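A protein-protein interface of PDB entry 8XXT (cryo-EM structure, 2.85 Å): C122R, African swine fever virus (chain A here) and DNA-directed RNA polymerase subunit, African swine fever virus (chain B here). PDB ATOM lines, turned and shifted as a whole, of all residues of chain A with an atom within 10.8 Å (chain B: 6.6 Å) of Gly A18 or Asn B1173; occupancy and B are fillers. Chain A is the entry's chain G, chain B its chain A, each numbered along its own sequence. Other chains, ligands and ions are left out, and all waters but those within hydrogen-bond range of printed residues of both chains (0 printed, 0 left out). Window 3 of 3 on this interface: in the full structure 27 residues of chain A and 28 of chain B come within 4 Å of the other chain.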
ATOM      1  N   ARG A  13      27.869 -25.735  12.745  1.00  0.00           N
ATOM      2  CA  ARG A  13      27.367 -26.015  11.405  1.00  0.00           C
ATOM      3  C   ARG A  13      28.079 -27.195  10.747  1.00  0.00           C
ATOM      4  O   ARG A  13      27.418 -28.123  10.275  1.00  0.00           O
ATOM      5  CB  ARG A  13      27.468 -24.759  10.538  1.00  0.00           C
ATOM      6  CG  ARG A  13      26.174 -23.960  10.520  1.00  0.00           C
ATOM      7  CD  ARG A  13      26.335 -22.614   9.835  1.00  0.00           C
ATOM      8  NE  ARG A  13      25.082 -22.122   9.274  1.00  0.00           N
ATOM      9  CZ  ARG A  13      24.439 -22.679   8.257  1.00  0.00           C
ATOM     10  NH1 ARG A  13      24.919 -23.741   7.631  1.00  0.00           N
ATOM     11  NH2 ARG A  13      23.288 -22.152   7.850  1.00  0.00           N
ATOM     12  N   THR A  14      29.413 -27.178  10.705  1.00  0.00           N
ATOM     13  CA  THR A  14      30.210 -28.345  10.313  1.00  0.00           C
ATOM     14  C   THR A  14      29.822 -28.804   8.899  1.00  0.00           C
ATOM     15  O   THR A  14      29.083 -29.769   8.686  1.00  0.00           O
ATOM     16  CB  THR A  14      30.081 -29.451  11.375  1.00  0.00           C
ATOM     17  OG1 THR A  14      30.933 -29.127  12.479  1.00  0.00           O
ATOM     18  CG2 THR A  14      30.570 -30.806  10.858  1.00  0.00           C
ATOM     19  N   TYR A  15      30.242 -27.995   7.926  1.00  0.00           N
ATOM     20  CA  TYR A  15      29.974 -28.314   6.528  1.00  0.00           C
ATOM     21  C   TYR A  15      30.846 -29.468   6.050  1.00  0.00           C
ATOM     22  O   TYR A  15      31.876 -29.243   5.406  1.00  0.00           O
ATOM     23  CB  TYR A  15      30.223 -27.107   5.624  1.00  0.00           C
ATOM     24  CG  TYR A  15      29.738 -25.788   6.163  1.00  0.00           C
ATOM     25  CD1 TYR A  15      30.561 -25.001   6.954  1.00  0.00           C
ATOM     26  CD2 TYR A  15      28.469 -25.318   5.863  1.00  0.00           C
ATOM     27  CE1 TYR A  15      30.129 -23.792   7.442  1.00  0.00           C
ATOM     28  CE2 TYR A  15      28.027 -24.108   6.349  1.00  0.00           C
ATOM     29  CZ  TYR A  15      28.863 -23.348   7.138  1.00  0.00           C
ATOM     30  OH  TYR A  15      28.438 -22.137   7.627  1.00  0.00           O
ATOM     31  N   VAL A  16      30.451 -30.701   6.359  1.00  0.00           N
ATOM     32  CA  VAL A  16      31.154 -31.894   5.898  1.00  0.00           C
ATOM     33  C   VAL A  16      30.121 -32.907   5.426  1.00  0.00           C
ATOM     34  O   VAL A  16      29.192 -33.241   6.168  1.00  0.00           O
ATOM     35  CB  VAL A  16      32.041 -32.506   7.001  1.00  0.00           C
ATOM     36  CG1 VAL A  16      32.635 -33.824   6.537  1.00  0.00           C
ATOM     37  CG2 VAL A  16      33.146 -31.541   7.398  1.00  0.00           C
ATOM     38  N   ASP A  17      30.273 -33.387   4.195  1.00  0.00           N
ATOM     39  CA  ASP A  17      31.280 -32.948   3.236  1.00  0.00           C
ATOM     40  C   ASP A  17      30.592 -32.263   2.061  1.00  0.00           C
ATOM     41  O   ASP A  17      30.949 -31.149   1.682  1.00  0.00           O
ATOM     42  CB  ASP A  17      32.132 -34.127   2.757  1.00  0.00           C
ATOM     43  CG  ASP A  17      31.295 -35.316   2.322  1.00  0.00           C
ATOM     44  OD1 ASP A  17      30.051 -35.232   2.397  1.00  0.00           O
ATOM     45  OD2 ASP A  17      31.882 -36.337   1.906  1.00  0.00           O
ATOM     46  N   GLY A  18      29.602 -32.945   1.490  1.00  0.00           N
ATOM     47  CA  GLY A  18      28.729 -32.359   0.496  1.00  0.00           C
ATOM     48  C   GLY A  18      27.414 -31.857   1.042  1.00  0.00           C
ATOM     49  O   GLY A  18      26.551 -31.447   0.254  1.00  0.00           O
ATOM     50  N   ASN A  19      27.221 -31.867   2.360  1.00  0.00           N
ATOM     51  CA  ASN A  19      25.968 -31.458   2.973  1.00  0.00           C
ATOM     52  C   ASN A  19      26.263 -30.713   4.267  1.00  0.00           C
ATOM     53  O   ASN A  19      27.411 -30.607   4.704  1.00  0.00           O
ATOM     54  CB  ASN A  19      25.054 -32.661   3.239  1.00  0.00           C
ATOM     55  CG  ASN A  19      23.595 -32.272   3.340  1.00  0.00           C
ATOM     56  OD1 ASN A  19      23.232 -31.121   3.106  1.00  0.00           O
ATOM     57  ND2 ASN A  19      22.750 -33.231   3.696  1.00  0.00           N
ATOM     58  N   ILE A  20      25.200 -30.200   4.881  1.00  0.00           N
ATOM     59  CA  ILE A  20      25.275 -29.413   6.107  1.00  0.00           C
ATOM     60  C   ILE A  20      24.712 -30.262   7.239  1.00  0.00           C
ATOM     61  O   ILE A  20      23.547 -30.679   7.193  1.00  0.00           O
ATOM     62  CB  ILE A  20      24.514 -28.086   5.960  1.00  0.00           C
ATOM     63  CG1 ILE A  20      24.270 -27.431   7.321  1.00  0.00           C
ATOM     64  CG2 ILE A  20      23.213 -28.288   5.196  1.00  0.00           C
ATOM     65  CD1 ILE A  20      25.531 -27.040   8.046  1.00  0.00           C
ATOM     66  N   ILE A  21      25.535 -30.523   8.253  1.00  0.00           N
ATOM     67  CA  ILE A  21      25.174 -31.410   9.356  1.00  0.00           C
ATOM     68  C   ILE A  21      25.459 -30.685  10.665  1.00  0.00           C
ATOM     69  O   ILE A  21      26.622 -30.519  11.050  1.00  0.00           O
ATOM     70  CB  ILE A  21      25.923 -32.750   9.290  1.00  0.00           C
ATOM     71  CG1 ILE A  21      25.857 -33.479  10.634  1.00  0.00           C
ATOM     72  CG2 ILE A  21      27.361 -32.551   8.829  1.00  0.00           C
ATOM     73  CD1 ILE A  21      26.481 -34.855  10.610  1.00  0.00           C
ATOM     74  N   GLN A  31      21.430 -32.789  10.939  1.00  0.00           N
ATOM     75  CA  GLN A  31      21.664 -32.524   9.522  1.00  0.00           C
ATOM     76  C   GLN A  31      20.885 -31.302   9.057  1.00  0.00           C
ATOM     77  O   GLN A  31      20.371 -30.534   9.876  1.00  0.00           O
ATOM     78  CB  GLN A  31      21.294 -33.737   8.660  1.00  0.00           C
ATOM     79  CG  GLN A  31      22.014 -35.016   9.033  1.00  0.00           C
ATOM     80  CD  GLN A  31      23.344 -35.161   8.325  1.00  0.00           C
ATOM     81  OE1 GLN A  31      23.718 -34.327   7.501  1.00  0.00           O
ATOM     82  NE2 GLN A  31      24.068 -36.227   8.642  1.00  0.00           N
ATOM     83  N   GLY A  32      20.798 -31.111   7.745  1.00  0.00           N
ATOM     84  CA  GLY A  32      20.088 -29.978   7.192  1.00  0.00           C
ATOM     85  C   GLY A  32      19.864 -30.115   5.704  1.00  0.00           C
ATOM     86  O   GLY A  32      20.760 -30.542   4.971  1.00  0.00           O
ATOM     87  N   ASP A  33      18.669 -29.764   5.244  1.00  0.00           N
ATOM     88  CA  ASP A  33      18.298 -29.895   3.845  1.00  0.00           C
ATOM     89  C   ASP A  33      17.905 -28.541   3.275  1.00  0.00           C
ATOM     90  O   ASP A  33      17.208 -27.761   3.930  1.00  0.00           O
ATOM     91  CB  ASP A  33      17.139 -30.880   3.678  1.00  0.00           C
ATOM     92  CG  ASP A  33      17.513 -32.294   4.076  1.00  0.00           C
ATOM     93  OD1 ASP A  33      18.723 -32.591   4.161  1.00  0.00           O
ATOM     94  OD2 ASP A  33      16.595 -33.107   4.309  1.00  0.00           O
ATOM     95  N   SER A  34      18.374 -28.265   2.058  1.00  0.00           N
ATOM     96  CA  SER A  34      17.910 -27.130   1.269  1.00  0.00           C
ATOM     97  C   SER A  34      18.056 -25.790   1.984  1.00  0.00           C
ATOM     98  O   SER A  34      19.041 -25.075   1.774  1.00  0.00           O
ATOM     99  CB  SER A  34      16.450 -27.351   0.866  1.00  0.00           C
ATOM    100  OG  SER A  34      15.742 -26.127   0.807  1.00  0.00           O
ATOM    101  N   ASN A  36      19.017 -24.733   4.684  1.00  0.00           N
ATOM    102  CA  ASN A  36      20.116 -24.491   5.606  1.00  0.00           C
ATOM    103  C   ASN A  36      21.397 -24.059   4.905  1.00  0.00           C
ATOM    104  O   ASN A  36      22.408 -23.834   5.577  1.00  0.00           O
ATOM    105  CB  ASN A  36      20.390 -25.743   6.443  1.00  0.00           C
ATOM    106  CG  ASN A  36      19.226 -26.114   7.333  1.00  0.00           C
ATOM    107  OD1 ASN A  36      19.051 -25.548   8.411  1.00  0.00           O
ATOM    108  ND2 ASN A  36      18.422 -27.071   6.887  1.00  0.00           N
ATOM    109  N   LEU A  37      21.379 -23.930   3.579  1.00  0.00           N
ATOM    110  CA  LEU A  37      22.600 -23.698   2.820  1.00  0.00           C
ATOM    111  C   LEU A  37      23.022 -22.235   2.777  1.00  0.00           C
ATOM    112  O   LEU A  37      24.111 -21.940   2.274  1.00  0.00           O
ATOM    113  CB  LEU A  37      22.432 -24.228   1.395  1.00  0.00           C
ATOM    114  CG  LEU A  37      22.158 -25.730   1.302  1.00  0.00           C
ATOM    115  CD1 LEU A  37      21.612 -26.104  -0.065  1.00  0.00           C
ATOM    116  CD2 LEU A  37      23.410 -26.525   1.621  1.00  0.00           C
ATOM    117  N   LEU A  38      22.204 -21.319   3.284  1.00  0.00           N
ATOM    118  CA  LEU A  38      22.563 -19.903   3.313  1.00  0.00           C
ATOM    119  C   LEU A  38      23.621 -19.687   4.384  1.00  0.00           C
ATOM    120  O   LEU A  38      23.312 -19.618   5.575  1.00  0.00           O
ATOM    121  CB  LEU A  38      21.332 -19.046   3.577  1.00  0.00           C
ATOM    122  CG  LEU A  38      21.484 -17.545   3.332  1.00  0.00           C
ATOM    123  CD1 LEU A  38      21.936 -17.280   1.909  1.00  0.00           C
ATOM    124  CD2 LEU A  38      20.178 -16.826   3.624  1.00  0.00           C
ATOM    125  N   VAL A  39      24.879 -19.574   3.965  1.00  0.00           N
ATOM    126  CA  VAL A  39      25.965 -19.397   4.921  1.00  0.00           C
ATOM    127  C   VAL A  39      25.992 -17.968   5.443  1.00  0.00           C
ATOM    128  O   VAL A  39      25.999 -17.734   6.657  1.00  0.00           O
ATOM    129  CB  VAL A  39      27.306 -19.794   4.280  1.00  0.00           C
ATOM    130  CG1 VAL A  39      28.457 -19.027   4.914  1.00  0.00           C
ATOM    131  CG2 VAL A  39      27.527 -21.284   4.402  1.00  0.00           C
ATOM    132  N   LEU B1132      26.294 -19.228  -0.643  1.00  0.00           N
ATOM    133  CA  LEU B1132      25.557 -20.480  -0.611  1.00  0.00           C
ATOM    134  C   LEU B1132      26.522 -21.654  -0.552  1.00  0.00           C
ATOM    135  O   LEU B1132      27.639 -21.589  -1.074  1.00  0.00           O
ATOM    136  CB  LEU B1132      24.648 -20.617  -1.835  1.00  0.00           C
ATOM    137  CG  LEU B1132      23.337 -19.831  -1.828  1.00  0.00           C
ATOM    138  CD1 LEU B1132      22.679 -19.909  -0.467  1.00  0.00           C
ATOM    139  CD2 LEU B1132      23.557 -18.388  -2.234  1.00  0.00           C
ATOM    140  N   TYR B1133      26.082 -22.732   0.097  1.00  0.00           N
ATOM    141  CA  TYR B1133      26.869 -23.958   0.198  1.00  0.00           C
ATOM    142  C   TYR B1133      26.377 -24.934  -0.865  1.00  0.00           C
ATOM    143  O   TYR B1133      25.636 -25.876  -0.593  1.00  0.00           O
ATOM    144  CB  TYR B1133      26.771 -24.551   1.598  1.00  0.00           C
ATOM    145  CG  TYR B1133      27.635 -25.774   1.800  1.00  0.00           C
ATOM    146  CD1 TYR B1133      29.009 -25.660   1.953  1.00  0.00           C
ATOM    147  CD2 TYR B1133      27.076 -27.044   1.840  1.00  0.00           C
ATOM    148  CE1 TYR B1133      29.802 -26.775   2.133  1.00  0.00           C
ATOM    149  CE2 TYR B1133      27.862 -28.164   2.022  1.00  0.00           C
ATOM    150  CZ  TYR B1133      29.223 -28.024   2.169  1.00  0.00           C
ATOM    151  OH  TYR B1133      30.008 -29.137   2.352  1.00  0.00           O
ATOM    152  N   GLU B1134      26.804 -24.698  -2.102  1.00  0.00           N
ATOM    153  CA  GLU B1134      26.399 -25.560  -3.201  1.00  0.00           C
ATOM    154  C   GLU B1134      27.481 -25.576  -4.269  1.00  0.00           C
ATOM    155  O   GLU B1134      28.213 -24.600  -4.452  1.00  0.00           O
ATOM    156  CB  GLU B1134      25.062 -25.112  -3.800  1.00  0.00           C
ATOM    157  CG  GLU B1134      24.845 -23.616  -3.780  1.00  0.00           C
ATOM    158  CD  GLU B1134      23.382 -23.247  -3.862  1.00  0.00           C
ATOM    159  OE1 GLU B1134      22.576 -23.870  -3.142  1.00  0.00           O
ATOM    160  OE2 GLU B1134      23.037 -22.337  -4.644  1.00  0.00           O
ATOM    161  N   THR B1135      27.577 -26.704  -4.963  1.00  0.00           N
ATOM    162  CA  THR B1135      28.493 -26.896  -6.075  1.00  0.00           C
ATOM    163  C   THR B1135      27.700 -26.954  -7.375  1.00  0.00           C
ATOM    164  O   THR B1135      26.479 -26.777  -7.395  1.00  0.00           O
ATOM    165  CB  THR B1135      29.322 -28.168  -5.882  1.00  0.00           C
ATOM    166  OG1 THR B1135      30.281 -28.284  -6.939  1.00  0.00           O
ATOM    167  CG2 THR B1135      28.425 -29.395  -5.894  1.00  0.00           C
ATOM    168  N   TYR B1136      28.407 -27.202  -8.474  1.00  0.00           N
ATOM    169  CA  TYR B1136      27.766 -27.341  -9.773  1.00  0.00           C
ATOM    170  C   TYR B1136      28.443 -28.446 -10.566  1.00  0.00           C
ATOM    171  O   TYR B1136      29.660 -28.417 -10.769  1.00  0.00           O
ATOM    172  CB  TYR B1136      27.802 -26.029 -10.561  1.00  0.00           C
ATOM    173  CG  TYR B1136      26.671 -25.902 -11.555  1.00  0.00           C
ATOM    174  CD1 TYR B1136      25.350 -25.878 -11.131  1.00  0.00           C
ATOM    175  CD2 TYR B1136      26.923 -25.812 -12.916  1.00  0.00           C
ATOM    176  CE1 TYR B1136      24.313 -25.766 -12.034  1.00  0.00           C
ATOM    177  CE2 TYR B1136      25.893 -25.698 -13.827  1.00  0.00           C
ATOM    178  CZ  TYR B1136      24.591 -25.676 -13.380  1.00  0.00           C
ATOM    179  OH  TYR B1136      23.561 -25.562 -14.286  1.00  0.00           O
ATOM    180  N   VAL B1143      20.535 -29.963  -6.888  1.00  0.00           N
ATOM    181  CA  VAL B1143      20.769 -29.682  -5.471  1.00  0.00           C
ATOM    182  C   VAL B1143      21.219 -28.235  -5.313  1.00  0.00           C
ATOM    183  O   VAL B1143      22.398 -27.914  -5.492  1.00  0.00           O
ATOM    184  CB  VAL B1143      21.787 -30.653  -4.845  1.00  0.00           C
ATOM    185  CG1 VAL B1143      21.988 -30.326  -3.373  1.00  0.00           C
ATOM    186  CG2 VAL B1143      21.321 -32.089  -5.013  1.00  0.00           C
ATOM    187  N   ILE B1171      35.027 -27.817  -9.158  1.00  0.00           N
ATOM    188  CA  ILE B1171      34.144 -26.831  -8.542  1.00  0.00           C
ATOM    189  C   ILE B1171      33.912 -27.214  -7.086  1.00  0.00           C
ATOM    190  O   ILE B1171      33.458 -28.324  -6.785  1.00  0.00           O
ATOM    191  CB  ILE B1171      32.818 -26.728  -9.301  1.00  0.00           C
ATOM    192  CG1 ILE B1171      33.032 -26.074 -10.662  1.00  0.00           C
ATOM    193  CG2 ILE B1171      31.808 -25.939  -8.492  1.00  0.00           C
ATOM    194  CD1 ILE B1171      31.747 -25.777 -11.386  1.00  0.00           C
ATOM    195  N   ALA B1172      34.211 -26.290  -6.177  1.00  0.00           N
ATOM    196  CA  ALA B1172      34.016 -26.529  -4.759  1.00  0.00           C
ATOM    197  C   ALA B1172      32.547 -26.357  -4.383  1.00  0.00           C
ATOM    198  O   ALA B1172      31.744 -25.789  -5.126  1.00  0.00           O
ATOM    199  CB  ALA B1172      34.893 -25.594  -3.930  1.00  0.00           C
ATOM    200  N   ASN B1173      32.199 -26.856  -3.199  1.00  0.00           N
ATOM    201  CA  ASN B1173      30.815 -26.831  -2.745  1.00  0.00           C
ATOM    202  C   ASN B1173      30.472 -25.487  -2.116  1.00  0.00           C
ATOM    203  O   ASN B1173      29.966 -25.432  -0.992  1.00  0.00           O
ATOM    204  CB  ASN B1173      30.568 -27.967  -1.751  1.00  0.00           C
ATOM    205  CG  ASN B1173      29.187 -28.568  -1.881  1.00  0.00           C
ATOM    206  OD1 ASN B1173      28.214 -27.867  -2.151  1.00  0.00           O
ATOM    207  ND2 ASN B1173      29.094 -29.877  -1.698  1.00  0.00           N
ATOM    208  N   TRP B1174      30.746 -24.398  -2.832  1.00  0.00           N
ATOM    209  CA  TRP B1174      30.433 -23.059  -2.355  1.00  0.00           C
ATOM    210  C   TRP B1174      30.071 -22.195  -3.551  1.00  0.00           C
ATOM    211  O   TRP B1174      30.459 -22.490  -4.685  1.00  0.00           O
ATOM    212  CB  TRP B1174      31.598 -22.422  -1.591  1.00  0.00           C
ATOM    213  CG  TRP B1174      32.092 -23.237  -0.445  1.00  0.00           C
ATOM    214  CD1 TRP B1174      32.870 -24.354  -0.509  1.00  0.00           C
ATOM    215  CD2 TRP B1174      31.799 -23.030   0.939  1.00  0.00           C
ATOM    216  NE1 TRP B1174      33.105 -24.837   0.753  1.00  0.00           N
ATOM    217  CE2 TRP B1174      32.454 -24.044   1.660  1.00  0.00           C
ATOM    218  CE3 TRP B1174      31.053 -22.079   1.641  1.00  0.00           C
ATOM    219  CZ2 TRP B1174      32.389 -24.135   3.044  1.00  0.00           C
ATOM    220  CZ3 TRP B1174      30.991 -22.169   3.013  1.00  0.00           C
ATOM    221  CH2 TRP B1174      31.653 -23.191   3.700  1.00  0.00           C
ATOM    222  N   CYS B1175      29.325 -21.124  -3.290  1.00  0.00           N
ATOM    223  CA  CYS B1175      28.922 -20.224  -4.360  1.00  0.00           C
ATOM    224  C   CYS B1175      28.452 -18.908  -3.762  1.00  0.00           C
ATOM    225  O   CYS B1175      27.769 -18.897  -2.736  1.00  0.00           O
ATOM    226  CB  CYS B1175      27.809 -20.836  -5.217  1.00  0.00           C
ATOM    227  SG  CYS B1175      27.086 -19.701  -6.416  1.00  0.00           S
ATOM    228  N   LEU B1227      33.551 -21.481  -6.606  1.00  0.00           N
ATOM    229  CA  LEU B1227      34.917 -21.654  -6.145  1.00  0.00           C
ATOM    230  C   LEU B1227      35.484 -22.976  -6.638  1.00  0.00           C
ATOM    231  O   LEU B1227      34.757 -23.961  -6.792  1.00  0.00           O
ATOM    232  CB  LEU B1227      34.984 -21.598  -4.619  1.00  0.00           C
ATOM    233  CG  LEU B1227      34.782 -20.220  -3.991  1.00  0.00           C
ATOM    234  CD1 LEU B1227      35.468 -19.171  -4.844  1.00  0.00           C
ATOM    235  CD2 LEU B1227      33.308 -19.900  -3.792  1.00  0.00           C
ATOM    236  N   GLU B1229      38.737 -25.991  -6.207  1.00  0.00           N
ATOM    237  CA  GLU B1229      39.521 -26.607  -5.139  1.00  0.00           C
ATOM    238  C   GLU B1229      40.785 -25.819  -4.825  1.00  0.00           C
ATOM    239  O   GLU B1229      41.248 -25.829  -3.679  1.00  0.00           O
ATOM    240  CB  GLU B1229      39.873 -28.056  -5.495  1.00  0.00           C
ATOM    241  CG  GLU B1229      38.700 -28.994  -5.789  1.00  0.00           C
ATOM    242  CD  GLU B1229      37.397 -28.553  -5.152  1.00  0.00           C
ATOM    243  OE1 GLU B1229      36.427 -28.286  -5.888  1.00  0.00           O
ATOM    244  OE2 GLU B1229      37.338 -28.508  -3.904  1.00  0.00           O
ATOM    245  N   PHE B1232      40.178 -23.454  -1.874  1.00  0.00           N
ATOM    246  CA  PHE B1232      40.076 -24.030  -0.541  1.00  0.00           C
ATOM    247  C   PHE B1232      41.240 -24.940  -0.185  1.00  0.00           C
ATOM    248  O   PHE B1232      41.272 -25.475   0.927  1.00  0.00           O
ATOM    249  CB  PHE B1232      38.759 -24.793  -0.398  1.00  0.00           C
ATOM    250  CG  PHE B1232      37.558 -23.906  -0.400  1.00  0.00           C
ATOM    251  CD1 PHE B1232      37.234 -23.164   0.720  1.00  0.00           C
ATOM    252  CD2 PHE B1232      36.764 -23.797  -1.524  1.00  0.00           C
ATOM    253  CE1 PHE B1232      36.133 -22.335   0.722  1.00  0.00           C
ATOM    254  CE2 PHE B1232      35.661 -22.974  -1.527  1.00  0.00           C
ATOM    255  CZ  PHE B1232      35.346 -22.240  -0.403  1.00  0.00           C
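Asn B1173 touches just one residue of chain A: Gly A18.
Tyr B1133 touches five residues of chain A.
No residue of chain A comes within 4 Å of Thr B1135.
No residue of chain A comes within 4 Å of Ala B1172.
Printed residues of chain A within 4 Å of Leu B1132: Leu A37 (3.5 Å) and Leu A38 (3.6 Å).
Printed residues of chain B within 4 Å of Tyr A15: Tyr B1133 (3.5 Å) and Trp B1174 (3.9 Å).
Asn A36 touches none of the printed residues of chain B.
The nearest residue of chain B that does not touch Gly A18 is Val B1143 (5.9 Å).
Printed residues of chain A that touch a printed residue of chain B: Tyr A15, Asp A17, Gly A18, Asn A19, Leu A37, Leu A38 and Val A39.
Hydrophobic or aromatic side chains of chain A within 4 Å of the printed part of chain B: Tyr A15, Leu A37, Leu A38 and Val A39.
Hydrophobic or aromatic side chains of chain B within 4 Å of the printed part of chain A: Leu B1132, Tyr B1133 and Trp B1174.
Tyr B1133 touches Tyr A15 (CE1 to CB, 3.5 Å).
CH2 of Trp B1174 touches CD1 of Tyr A15, 3.9 Å away.
Gly A18 touches Tyr B1133 (C to CE2, 3.8 Å).
ND2 of Asn B1173 touches CA of Gly A18, 3.3 Å away.
Tyr B1133 touches Asn A19 (CE2 to O, 3.7 Å).
Leu B1132 touches Leu A37 (CA to O, 3.5 Å).
CD1 of Leu A37 touches OE1 of Glu B1134, 3.9 Å away.
Leu A38 touches Leu B1132 (CD1 to CD1, 3.6 Å).
Trp B1174 touches Val A39 (CZ3 to CG2, 3.8 Å).
The backbone NH of Leu B1132 is in hydrogen-bond range of the backbone carbonyl oxygen of Cys B1175, at 2.6 Å.
N of Glu B1134 lies within hydrogen-bond range of O of Asn B1173, at 3.4 Å.
The backbone carbonyl oxygen (O) of Glu B1134 sits at hydrogen-bond distance from the backbone NH (N) of Trp B1174 (3.0 Å).
The side-chain amide oxygen (OD1) of Asn B1173 sits at hydrogen-bond distance from the backbone NH (N) of Thr B1135.
The backbone carbonyl oxygen (O) of Leu A38 is in hydrogen-bond range of the guanidinium group (NH2) of Arg A13 (3.4 Å).
The side-chain amide oxygen (OD1) of Asn A19 sits close to the backbone carbonyl oxygen (O) of Gly A32 (3.2 Å).
N of Tyr B1133 is in hydrogen-bond range of O of Leu A37, at 3.0 Å.
O of Asp A17 sits close to OH of Tyr B1133, at 2.3 Å.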
